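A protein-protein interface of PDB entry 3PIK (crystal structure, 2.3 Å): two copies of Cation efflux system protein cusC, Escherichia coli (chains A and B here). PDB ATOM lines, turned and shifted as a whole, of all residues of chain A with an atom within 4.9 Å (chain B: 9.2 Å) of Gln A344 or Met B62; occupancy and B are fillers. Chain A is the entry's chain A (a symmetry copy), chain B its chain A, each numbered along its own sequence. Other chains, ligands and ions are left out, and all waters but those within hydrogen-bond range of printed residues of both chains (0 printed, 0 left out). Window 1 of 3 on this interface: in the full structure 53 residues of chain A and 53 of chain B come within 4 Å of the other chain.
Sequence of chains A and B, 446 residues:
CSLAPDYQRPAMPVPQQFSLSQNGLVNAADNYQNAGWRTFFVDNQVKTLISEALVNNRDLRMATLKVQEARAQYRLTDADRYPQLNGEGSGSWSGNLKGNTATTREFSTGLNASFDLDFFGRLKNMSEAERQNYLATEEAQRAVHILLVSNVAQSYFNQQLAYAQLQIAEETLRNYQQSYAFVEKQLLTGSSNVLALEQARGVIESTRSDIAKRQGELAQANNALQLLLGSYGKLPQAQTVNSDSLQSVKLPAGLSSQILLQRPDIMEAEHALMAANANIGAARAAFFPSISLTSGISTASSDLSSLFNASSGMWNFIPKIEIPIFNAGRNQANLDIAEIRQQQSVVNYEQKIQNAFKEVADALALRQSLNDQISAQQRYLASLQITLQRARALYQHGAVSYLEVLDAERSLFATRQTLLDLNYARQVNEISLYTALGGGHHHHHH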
ATOM      1  N   ILE A 340      10.860  -1.919 -19.777  1.00  0.00           N
ATOM      2  CA  ILE A 340      11.877  -0.986 -20.234  1.00  0.00           C
ATOM      3  C   ILE A 340      11.610   0.386 -19.622  1.00  0.00           C
ATOM      4  O   ILE A 340      12.553   1.110 -19.279  1.00  0.00           O
ATOM      5  CB  ILE A 340      11.897  -0.870 -21.776  1.00  0.00           C
ATOM      6  CG1 ILE A 340      12.422  -2.171 -22.396  1.00  0.00           C
ATOM      7  CG2 ILE A 340      12.780   0.310 -22.201  1.00  0.00           C
ATOM      8  CD1 ILE A 340      12.166  -2.315 -23.892  1.00  0.00           C
ATOM      9  N   ARG A 341      10.325   0.721 -19.480  1.00  0.00           N
ATOM     10  CA  ARG A 341       9.901   2.000 -18.907  1.00  0.00           C
ATOM     11  C   ARG A 341      10.180   2.068 -17.420  1.00  0.00           C
ATOM     12  O   ARG A 341      10.387   3.148 -16.872  1.00  0.00           O
ATOM     13  CB  ARG A 341       8.412   2.265 -19.157  1.00  0.00           C
ATOM     14  CG  ARG A 341       8.143   2.944 -20.492  1.00  0.00           C
ATOM     15  CD  ARG A 341       6.658   3.179 -20.768  1.00  0.00           C
ATOM     16  NE  ARG A 341       6.481   3.742 -22.106  1.00  0.00           N
ATOM     17  CZ  ARG A 341       5.321   3.817 -22.749  1.00  0.00           C
ATOM     18  NH1 ARG A 341       4.206   3.355 -22.183  1.00  0.00           N
ATOM     19  NH2 ARG A 341       5.278   4.346 -23.967  1.00  0.00           N
ATOM     20  N   GLN A 342      10.171   0.909 -16.772  1.00  0.00           N
ATOM     21  CA  GLN A 342      10.479   0.840 -15.356  1.00  0.00           C
ATOM     22  C   GLN A 342      11.973   1.070 -15.202  1.00  0.00           C
ATOM     23  O   GLN A 342      12.406   1.760 -14.284  1.00  0.00           O
ATOM     24  CB  GLN A 342      10.070  -0.520 -14.783  1.00  0.00           C
ATOM     25  CG  GLN A 342      10.365  -0.711 -13.304  1.00  0.00           C
ATOM     26  CD  GLN A 342      11.099  -2.014 -13.029  1.00  0.00           C
ATOM     27  OE1 GLN A 342      12.080  -2.342 -13.703  1.00  0.00           O
ATOM     28  NE2 GLN A 342      10.611  -2.779 -12.049  1.00  0.00           N
ATOM     29  N   GLN A 343      12.754   0.501 -16.120  1.00  0.00           N
ATOM     30  CA  GLN A 343      14.183   0.748 -16.124  1.00  0.00           C
ATOM     31  C   GLN A 343      14.472   2.224 -16.377  1.00  0.00           C
ATOM     32  O   GLN A 343      15.436   2.772 -15.826  1.00  0.00           O
ATOM     33  CB  GLN A 343      14.903  -0.126 -17.159  1.00  0.00           C
ATOM     34  CG  GLN A 343      14.954  -1.610 -16.808  1.00  0.00           C
ATOM     35  CD  GLN A 343      15.607  -2.432 -17.918  1.00  0.00           C
ATOM     36  OE1 GLN A 343      15.217  -2.340 -19.085  1.00  0.00           O
ATOM     37  NE2 GLN A 343      16.614  -3.225 -17.561  1.00  0.00           N
ATOM     38  N   GLN A 344      13.639   2.866 -17.203  1.00  0.00           N
ATOM     39  CA  GLN A 344      13.807   4.298 -17.471  1.00  0.00           C
ATOM     40  C   GLN A 344      13.555   5.112 -16.206  1.00  0.00           C
ATOM     41  O   GLN A 344      14.259   6.076 -15.942  1.00  0.00           O
ATOM     42  CB  GLN A 344      12.895   4.789 -18.606  1.00  0.00           C
ATOM     43  CG  GLN A 344      13.342   4.405 -20.023  1.00  0.00           C
ATOM     44  CD  GLN A 344      12.318   4.820 -21.086  1.00  0.00           C
ATOM     45  OE1 GLN A 344      12.267   5.975 -21.509  1.00  0.00           O
ATOM     46  NE2 GLN A 344      11.506   3.879 -21.512  1.00  0.00           N
ATOM     47  N   SER A 345      12.553   4.702 -15.427  1.00  0.00           N
ATOM     48  CA  SER A 345      12.220   5.381 -14.187  1.00  0.00           C
ATOM     49  C   SER A 345      13.353   5.255 -13.187  1.00  0.00           C
ATOM     50  O   SER A 345      13.603   6.167 -12.422  1.00  0.00           O
ATOM     51  CB  SER A 345      10.944   4.794 -13.567  1.00  0.00           C
ATOM     52  OG  SER A 345       9.819   5.096 -14.355  1.00  0.00           O
ATOM     53  N   VAL A 346      14.017   4.103 -13.178  1.00  0.00           N
ATOM     54  CA  VAL A 346      15.171   3.899 -12.313  1.00  0.00           C
ATOM     55  C   VAL A 346      16.313   4.857 -12.677  1.00  0.00           C
ATOM     56  O   VAL A 346      16.921   5.463 -11.811  1.00  0.00           O
ATOM     57  CB  VAL A 346      15.681   2.457 -12.395  1.00  0.00           C
ATOM     58  CG1 VAL A 346      17.076   2.354 -11.771  1.00  0.00           C
ATOM     59  CG2 VAL A 346      14.693   1.496 -11.718  1.00  0.00           C
ATOM     60  N   VAL A 347      16.588   4.993 -13.966  1.00  0.00           N
ATOM     61  CA  VAL A 347      17.624   5.905 -14.430  1.00  0.00           C
ATOM     62  C   VAL A 347      17.242   7.360 -14.100  1.00  0.00           C
ATOM     63  O   VAL A 347      18.078   8.159 -13.653  1.00  0.00           O
ATOM     64  CB  VAL A 347      17.854   5.740 -15.946  1.00  0.00           C
ATOM     65  CG1 VAL A 347      18.886   6.753 -16.461  1.00  0.00           C
ATOM     66  CG2 VAL A 347      18.252   4.286 -16.284  1.00  0.00           C
ATOM     67  N   ASN A 348      15.977   7.696 -14.314  1.00  0.00           N
ATOM     68  CA  ASN A 348      15.460   9.029 -13.989  1.00  0.00           C
ATOM     69  C   ASN A 348      15.654   9.365 -12.521  1.00  0.00           C
ATOM     70  O   ASN A 348      16.114  10.455 -12.176  1.00  0.00           O
ATOM     71  CB  ASN A 348      13.978   9.116 -14.314  1.00  0.00           C
ATOM     72  CG  ASN A 348      13.371  10.442 -13.900  1.00  0.00           C
ATOM     73  OD1 ASN A 348      12.550  10.509 -12.984  1.00  0.00           O
ATOM     74  ND2 ASN A 348      13.769  11.504 -14.579  1.00  0.00           N
ATOM     75  N   GLN A 351      19.291  10.009 -12.007  1.00  0.00           N
ATOM     76  CA  GLN A 351      19.653  11.311 -12.554  1.00  0.00           C
ATOM     77  C   GLN A 351      19.267  12.423 -11.594  1.00  0.00           C
ATOM     78  O   GLN A 351      20.014  13.382 -11.390  1.00  0.00           O
ATOM     79  CB  GLN A 351      18.957  11.549 -13.899  1.00  0.00           C
ATOM     80  CG  GLN A 351      19.537  10.770 -15.071  1.00  0.00           C
ATOM     81  CD  GLN A 351      18.635  10.802 -16.312  1.00  0.00           C
ATOM     82  OE1 GLN A 351      17.420  10.626 -16.218  1.00  0.00           O
ATOM     83  NE2 GLN A 351      19.231  11.034 -17.468  1.00  0.00           N
ATOM     84  N   LEU B  54      31.026   6.794 -21.178  1.00  0.00           N
ATOM     85  CA  LEU B  54      30.285   5.897 -22.072  1.00  0.00           C
ATOM     86  C   LEU B  54      29.654   4.721 -21.338  1.00  0.00           C
ATOM     87  O   LEU B  54      28.646   4.182 -21.770  1.00  0.00           O
ATOM     88  CB  LEU B  54      31.166   5.395 -23.218  1.00  0.00           C
ATOM     89  CG  LEU B  54      31.621   6.560 -24.099  1.00  0.00           C
ATOM     90  CD1 LEU B  54      32.569   6.093 -25.213  1.00  0.00           C
ATOM     91  CD2 LEU B  54      30.404   7.285 -24.667  1.00  0.00           C
ATOM     92  N   VAL B  55      30.244   4.329 -20.224  1.00  0.00           N
ATOM     93  CA  VAL B  55      29.686   3.244 -19.445  1.00  0.00           C
ATOM     94  C   VAL B  55      28.632   3.739 -18.456  1.00  0.00           C
ATOM     95  O   VAL B  55      27.551   3.165 -18.356  1.00  0.00           O
ATOM     96  CB  VAL B  55      30.788   2.487 -18.662  1.00  0.00           C
ATOM     97  CG1 VAL B  55      30.183   1.358 -17.860  1.00  0.00           C
ATOM     98  CG2 VAL B  55      31.838   1.949 -19.615  1.00  0.00           C
ATOM     99  N   ASN B  56      28.947   4.793 -17.716  1.00  0.00           N
ATOM    100  CA  ASN B  56      28.149   5.116 -16.533  1.00  0.00           C
ATOM    101  C   ASN B  56      27.188   6.284 -16.687  1.00  0.00           C
ATOM    102  O   ASN B  56      26.317   6.479 -15.848  1.00  0.00           O
ATOM    103  CB  ASN B  56      29.066   5.372 -15.338  1.00  0.00           C
ATOM    104  CG  ASN B  56      29.834   4.126 -14.919  1.00  0.00           C
ATOM    105  OD1 ASN B  56      29.249   3.068 -14.680  1.00  0.00           O
ATOM    106  ND2 ASN B  56      31.155   4.246 -14.843  1.00  0.00           N
ATOM    107  N   ASN B  57      27.361   7.076 -17.737  1.00  0.00           N
ATOM    108  CA  ASN B  57      26.557   8.274 -17.893  1.00  0.00           C
ATOM    109  C   ASN B  57      25.064   7.974 -18.048  1.00  0.00           C
ATOM    110  O   ASN B  57      24.661   7.186 -18.903  1.00  0.00           O
ATOM    111  CB  ASN B  57      27.040   9.122 -19.061  1.00  0.00           C
ATOM    112  CG  ASN B  57      26.170  10.338 -19.276  1.00  0.00           C
ATOM    113  OD1 ASN B  57      25.179  10.278 -19.984  1.00  0.00           O
ATOM    114  ND2 ASN B  57      26.533  11.449 -18.648  1.00  0.00           N
ATOM    115  N   ARG B  58      24.262   8.637 -17.220  1.00  0.00           N
ATOM    116  CA  ARG B  58      22.831   8.376 -17.116  1.00  0.00           C
ATOM    117  C   ARG B  58      22.021   8.782 -18.350  1.00  0.00           C
ATOM    118  O   ARG B  58      21.121   8.046 -18.767  1.00  0.00           O
ATOM    119  CB  ARG B  58      22.261   9.046 -15.860  1.00  0.00           C
ATOM    120  CG  ARG B  58      22.713   8.396 -14.568  1.00  0.00           C
ATOM    121  CD  ARG B  58      23.501   7.115 -14.855  1.00  0.00           C
ATOM    122  NE  ARG B  58      22.738   5.941 -14.511  1.00  0.00           N
ATOM    123  CZ  ARG B  58      22.973   4.713 -14.974  1.00  0.00           C
ATOM    124  NH1 ARG B  58      23.966   4.476 -15.825  1.00  0.00           N
ATOM    125  NH2 ARG B  58      22.191   3.716 -14.575  1.00  0.00           N
ATOM    126  N   ASP B  59      22.342   9.938 -18.926  1.00  0.00           N
ATOM    127  CA  ASP B  59      21.655  10.425 -20.120  1.00  0.00           C
ATOM    128  C   ASP B  59      21.795   9.446 -21.267  1.00  0.00           C
ATOM    129  O   ASP B  59      20.842   9.201 -22.003  1.00  0.00           O
ATOM    130  CB  ASP B  59      22.214  11.785 -20.557  1.00  0.00           C
ATOM    131  CG  ASP B  59      21.686  12.933 -19.718  1.00  0.00           C
ATOM    132  OD1 ASP B  59      21.075  12.671 -18.663  1.00  0.00           O
ATOM    133  OD2 ASP B  59      21.890  14.102 -20.103  1.00  0.00           O
ATOM    134  N   LEU B  60      22.992   8.892 -21.420  1.00  0.00           N
ATOM    135  CA  LEU B  60      23.263   7.969 -22.513  1.00  0.00           C
ATOM    136  C   LEU B  60      22.573   6.629 -22.242  1.00  0.00           C
ATOM    137  O   LEU B  60      21.991   6.022 -23.135  1.00  0.00           O
ATOM    138  CB  LEU B  60      24.769   7.776 -22.712  1.00  0.00           C
ATOM    139  CG  LEU B  60      25.131   6.753 -23.797  1.00  0.00           C
ATOM    140  CD1 LEU B  60      24.599   7.181 -25.160  1.00  0.00           C
ATOM    141  CD2 LEU B  60      26.622   6.508 -23.864  1.00  0.00           C
ATOM    142  N   ARG B  61      22.634   6.182 -20.997  1.00  0.00           N
ATOM    143  CA  ARG B  61      21.909   4.994 -20.587  1.00  0.00           C
ATOM    144  C   ARG B  61      20.412   5.152 -20.903  1.00  0.00           C
ATOM    145  O   ARG B  61      19.765   4.239 -21.417  1.00  0.00           O
ATOM    146  CB  ARG B  61      22.136   4.741 -19.093  1.00  0.00           C
ATOM    147  CG  ARG B  61      21.363   3.569 -18.542  1.00  0.00           C
ATOM    148  CD  ARG B  61      21.601   2.294 -19.352  1.00  0.00           C
ATOM    149  NE  ARG B  61      20.871   1.169 -18.778  1.00  0.00           N
ATOM    150  CZ  ARG B  61      20.728  -0.011 -19.366  1.00  0.00           C
ATOM    151  NH1 ARG B  61      21.258  -0.229 -20.564  1.00  0.00           N
ATOM    152  NH2 ARG B  61      20.048  -0.966 -18.756  1.00  0.00           N
ATOM    153  N   MET B  62      19.873   6.331 -20.626  1.00  0.00           N
ATOM    154  CA  MET B  62      18.467   6.607 -20.905  1.00  0.00           C
ATOM    155  C   MET B  62      18.185   6.577 -22.412  1.00  0.00           C
ATOM    156  O   MET B  62      17.131   6.090 -22.859  1.00  0.00           O
ATOM    157  CB  MET B  62      18.077   7.969 -20.313  1.00  0.00           C
ATOM    158  CG  MET B  62      16.645   8.370 -20.574  1.00  0.00           C
ATOM    159  SD  MET B  62      15.490   7.379 -19.604  1.00  0.00           S
ATOM    160  CE  MET B  62      15.685   8.161 -18.001  1.00  0.00           C
ATOM    161  N   ALA B  63      19.126   7.102 -23.195  1.00  0.00           N
ATOM    162  CA  ALA B  63      18.974   7.094 -24.646  1.00  0.00           C
ATOM    163  C   ALA B  63      18.993   5.661 -25.180  1.00  0.00           C
ATOM    164  O   ALA B  63      18.277   5.323 -26.128  1.00  0.00           O
ATOM    165  CB  ALA B  63      20.066   7.935 -25.308  1.00  0.00           C
ATOM    166  N   THR B  64      19.804   4.814 -24.560  1.00  0.00           N
ATOM    167  CA  THR B  64      19.852   3.395 -24.925  1.00  0.00           C
ATOM    168  C   THR B  64      18.530   2.708 -24.610  1.00  0.00           C
ATOM    169  O   THR B  64      18.024   1.909 -25.396  1.00  0.00           O
ATOM    170  CB  THR B  64      20.990   2.667 -24.175  1.00  0.00           C
ATOM    171  OG1 THR B  64      22.238   3.260 -24.541  1.00  0.00           O
ATOM    172  CG2 THR B  64      21.026   1.174 -24.532  1.00  0.00           C
ATOM    173  N   LEU B  65      17.957   3.033 -23.457  1.00  0.00           N
ATOM    174  CA  LEU B  65      16.680   2.436 -23.084  1.00  0.00           C
ATOM    175  C   LEU B  65      15.564   2.872 -24.037  1.00  0.00           C
ATOM    176  O   LEU B  65      14.677   2.079 -24.360  1.00  0.00           O
ATOM    177  CB  LEU B  65      16.329   2.744 -21.630  1.00  0.00           C
ATOM    178  CG  LEU B  65      17.236   2.030 -20.618  1.00  0.00           C
ATOM    179  CD1 LEU B  65      16.967   2.519 -19.213  1.00  0.00           C
ATOM    180  CD2 LEU B  65      17.075   0.494 -20.690  1.00  0.00           C
ATOM    181  N   LYS B  66      15.623   4.114 -24.511  1.00  0.00           N
ATOM    182  CA  LYS B  66      14.617   4.603 -25.455  1.00  0.00           C
ATOM    183  C   LYS B  66      14.677   3.830 -26.771  1.00  0.00           C
ATOM    184  O   LYS B  66      13.657   3.604 -27.405  1.00  0.00           O
ATOM    185  CB  LYS B  66      14.771   6.101 -25.718  1.00  0.00           C
ATOM    186  CG  LYS B  66      14.150   6.994 -24.654  1.00  0.00           C
ATOM    187  CD  LYS B  66      14.505   8.444 -24.929  1.00  0.00           C
ATOM    188  CE  LYS B  66      14.034   9.371 -23.829  1.00  0.00           C
ATOM    189  NZ  LYS B  66      14.316  10.797 -24.202  1.00  0.00           N
ATOM    190  N   VAL B  67      15.876   3.427 -27.182  1.00  0.00           N
ATOM    191  CA  VAL B  67      15.995   2.579 -28.361  1.00  0.00           C
ATOM    192  C   VAL B  67      15.296   1.242 -28.130  1.00  0.00           C
ATOM    193  O   VAL B  67      14.593   0.756 -29.001  1.00  0.00           O
ATOM    194  CB  VAL B  67      17.453   2.318 -28.764  1.00  0.00           C
ATOM    195  CG1 VAL B  67      17.504   1.367 -29.982  1.00  0.00           C
ATOM    196  CG2 VAL B  67      18.168   3.630 -29.083  1.00  0.00           C
ATOM    197  N   GLN B  68      15.475   0.654 -26.952  1.00  0.00           N
ATOM    198  CA  GLN B  68      14.855  -0.636 -26.680  1.00  0.00           C
ATOM    199  C   GLN B  68      13.331  -0.520 -26.684  1.00  0.00           C
ATOM    200  O   GLN B  68      12.628  -1.372 -27.217  1.00  0.00           O
ATOM    201  CB  GLN B  68      15.361  -1.196 -25.364  1.00  0.00           C
ATOM    202  CG  GLN B  68      16.839  -1.565 -25.435  1.00  0.00           C
ATOM    203  CD  GLN B  68      17.411  -1.960 -24.085  1.00  0.00           C
ATOM    204  OE1 GLN B  68      18.629  -2.002 -23.905  1.00  0.00           O
ATOM    205  NE2 GLN B  68      16.531  -2.260 -23.129  1.00  0.00           N
ATOM    206  N   GLU B  69      12.848   0.567 -26.103  1.00  0.00           N
ATOM    207  CA  GLU B  69      11.436   0.854 -26.008  1.00  0.00           C
ATOM    208  C   GLU B  69      10.813   0.962 -27.397  1.00  0.00           C
ATOM    209  O   GLU B  69       9.759   0.390 -27.672  1.00  0.00           O
ATOM    210  CB  GLU B  69      11.268   2.178 -25.264  1.00  0.00           C
ATOM    211  CG  GLU B  69      10.011   2.255 -24.448  1.00  0.00           C
ATOM    212  CD  GLU B  69       9.025   3.236 -25.014  1.00  0.00           C
ATOM    213  OE1 GLU B  69       8.976   4.380 -24.489  1.00  0.00           O
ATOM    214  OE2 GLU B  69       8.304   2.858 -25.968  1.00  0.00           O
ATOM    215  N   ALA B  70      11.480   1.713 -28.264  1.00  0.00           N
ATOM    216  CA  ALA B  70      11.030   1.891 -29.626  1.00  0.00           C
ATOM    217  C   ALA B  70      11.091   0.566 -30.400  1.00  0.00           C
ATOM    218  O   ALA B  70      10.263   0.314 -31.268  1.00  0.00           O
ATOM    219  CB  ALA B  70      11.853   2.984 -30.323  1.00  0.00           C
ATOM    220  N   ALA B  72      10.586  -2.373 -29.047  1.00  0.00           N
ATOM    221  CA  ALA B  72       9.431  -3.102 -28.537  1.00  0.00           C
ATOM    222  C   ALA B  72       8.114  -2.569 -29.130  1.00  0.00           C
ATOM    223  O   ALA B  72       7.226  -3.341 -29.477  1.00  0.00           O
ATOM    224  CB  ALA B  72       9.406  -3.071 -26.992  1.00  0.00           C
ATOM    225  N   THR B 137      15.314   6.508 -33.607  1.00  0.00           N
ATOM    226  CA  THR B 137      15.645   6.506 -32.186  1.00  0.00           C
ATOM    227  C   THR B 137      17.088   5.998 -31.998  1.00  0.00           C
ATOM    228  O   THR B 137      17.833   6.510 -31.164  1.00  0.00           O
ATOM    229  CB  THR B 137      14.610   5.679 -31.364  1.00  0.00           C
ATOM    230  OG1 THR B 137      13.302   6.258 -31.512  1.00  0.00           O
ATOM    231  CG2 THR B 137      14.959   5.664 -29.892  1.00  0.00           C
ATOM    232  N   ALA B 140      19.253   8.916 -32.754  1.00  0.00           N
ATOM    233  CA  ALA B 140      19.221   9.893 -31.676  1.00  0.00           C
ATOM    234  C   ALA B 140      20.187   9.448 -30.583  1.00  0.00           C
ATOM    235  O   ALA B 140      20.916  10.251 -29.995  1.00  0.00           O
ATOM    236  CB  ALA B 140      17.782  10.032 -31.121  1.00  0.00           C
ATOM    237  N   GLN B 141      20.183   8.144 -30.341  1.00  0.00           N
ATOM    238  CA  GLN B 141      21.096   7.517 -29.415  1.00  0.00           C
ATOM    239  C   GLN B 141      22.546   7.800 -29.807  1.00  0.00           C
ATOM    240  O   GLN B 141      23.363   8.173 -28.969  1.00  0.00           O
ATOM    241  CB  GLN B 141      20.843   6.018 -29.406  1.00  0.00           C
ATOM    242  CG  GLN B 141      21.343   5.327 -28.155  1.00  0.00           C
ATOM    243  CD  GLN B 141      22.787   4.914 -28.241  1.00  0.00           C
ATOM    244  OE1 GLN B 141      23.354   4.415 -27.272  1.00  0.00           O
ATOM    245  NE2 GLN B 141      23.394   5.115 -29.400  1.00  0.00           N
ATOM    246  N   VAL B 144      23.413  11.351 -28.938  1.00  0.00           N
ATOM    247  CA  VAL B 144      23.704  11.551 -27.531  1.00  0.00           C
ATOM    248  C   VAL B 144      25.114  11.027 -27.228  1.00  0.00           C
ATOM    249  O   VAL B 144      25.855  11.602 -26.450  1.00  0.00           O
ATOM    250  CB  VAL B 144      22.674  10.821 -26.653  1.00  0.00           C
ATOM    251  CG1 VAL B 144      23.030  10.974 -25.179  1.00  0.00           C
ATOM    252  CG2 VAL B 144      21.285  11.368 -26.928  1.00  0.00           C
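Leu B65 touches Ile A340.
Ile A340 touches Gln B68 (CD1 to O, 3.5 Å).
Gln A343 touches Leu B65 (O to CD1, 3.7 Å).
Gln A344 touches Met B62.
Gln A344 touches Leu B65.
Val A347 touches Arg B58.
CG2 of Val A347 touches CG of Arg B61, at 3.9 Å.
Val A347 touches Met B62 (CG1 to CE, 3.8 Å).
Gln A351 touches Arg B58.
OE1 of Gln A351 touches CE of Met B62 (3.5 Å).
Gln A342 touches none of the printed residues of chain B.
Printed residues of chain B within 4 Å of Gln A343: Leu B65 (3.7 Å).
Gln A344 touches just these residues of chain B: Met B62 (3.3 Å), Leu B65 (3.8 Å), Lys B66 (3.8 Å) and Glu B69 (3.7 Å).
No residue of chain B comes within 4 Å of Ser A345.
Of the printed residues of chain B, Gln A351 touches Arg B58, Asp B59 and Met B62.
Printed residues of chain A within 4 Å of Asp B59: Gln A351 (2.7 Å).
Met B62 touches just these residues of chain A: Gln A344 (3.3 Å), Val A347 (3.8 Å), Asn A348 (3.7 Å) and Gln A351 (3.5 Å).
Val B67 touches none of the printed residues of chain A.
Of the printed residues of chain A, Glu B69 touches Ile A340, Arg A341 and Gln A344.
The nearest printed residue of chain A that does not touch Met B62 is Ser A345 (5.3 Å).
No position is printed for both chains.
Of the 17 pairs that touch across the chains among the printed residues, none has its exchanged pair printed and touching as well.
The side-chain carboxylate (OD1) of Asp B59 sits at hydrogen-bond distance from the side-chain amide nitrogen (NE2) of Gln A351 (2.7 Å).
OE1 of Glu B69 lies within salt-bridge range of NE of Arg A341 (3.5 Å).
NH1 of Arg B58 lies close to O of Asn B56, 3.1 Å away.
The side-chain amide oxygen (OD1) of Asn B57 sits at hydrogen-bond distance from the backbone NH (N) of Asp B59 (3.0 Å).
O of Arg A341 is in hydrogen-bond range of OG of Ser A345.
Hydrophobic or aromatic side chains of chain A within 4 Å of the printed part of chain B: Ile A340 and Val A347.
Of the 22 printed residues of chain B, 8 touch a printed residue of chain A.
Hydrophobic or aromatic side chains of chain B within 4 Å of the printed part of chain A: Met B62 and Leu B65.
Among the printed residues, 17 pairs touch across the chains.
Among the printed residues, Asp or Glu carboxylates within 4 Å of a Lys or Arg side-chain nitrogen of the other chain: Arg A341 with Glu B69.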
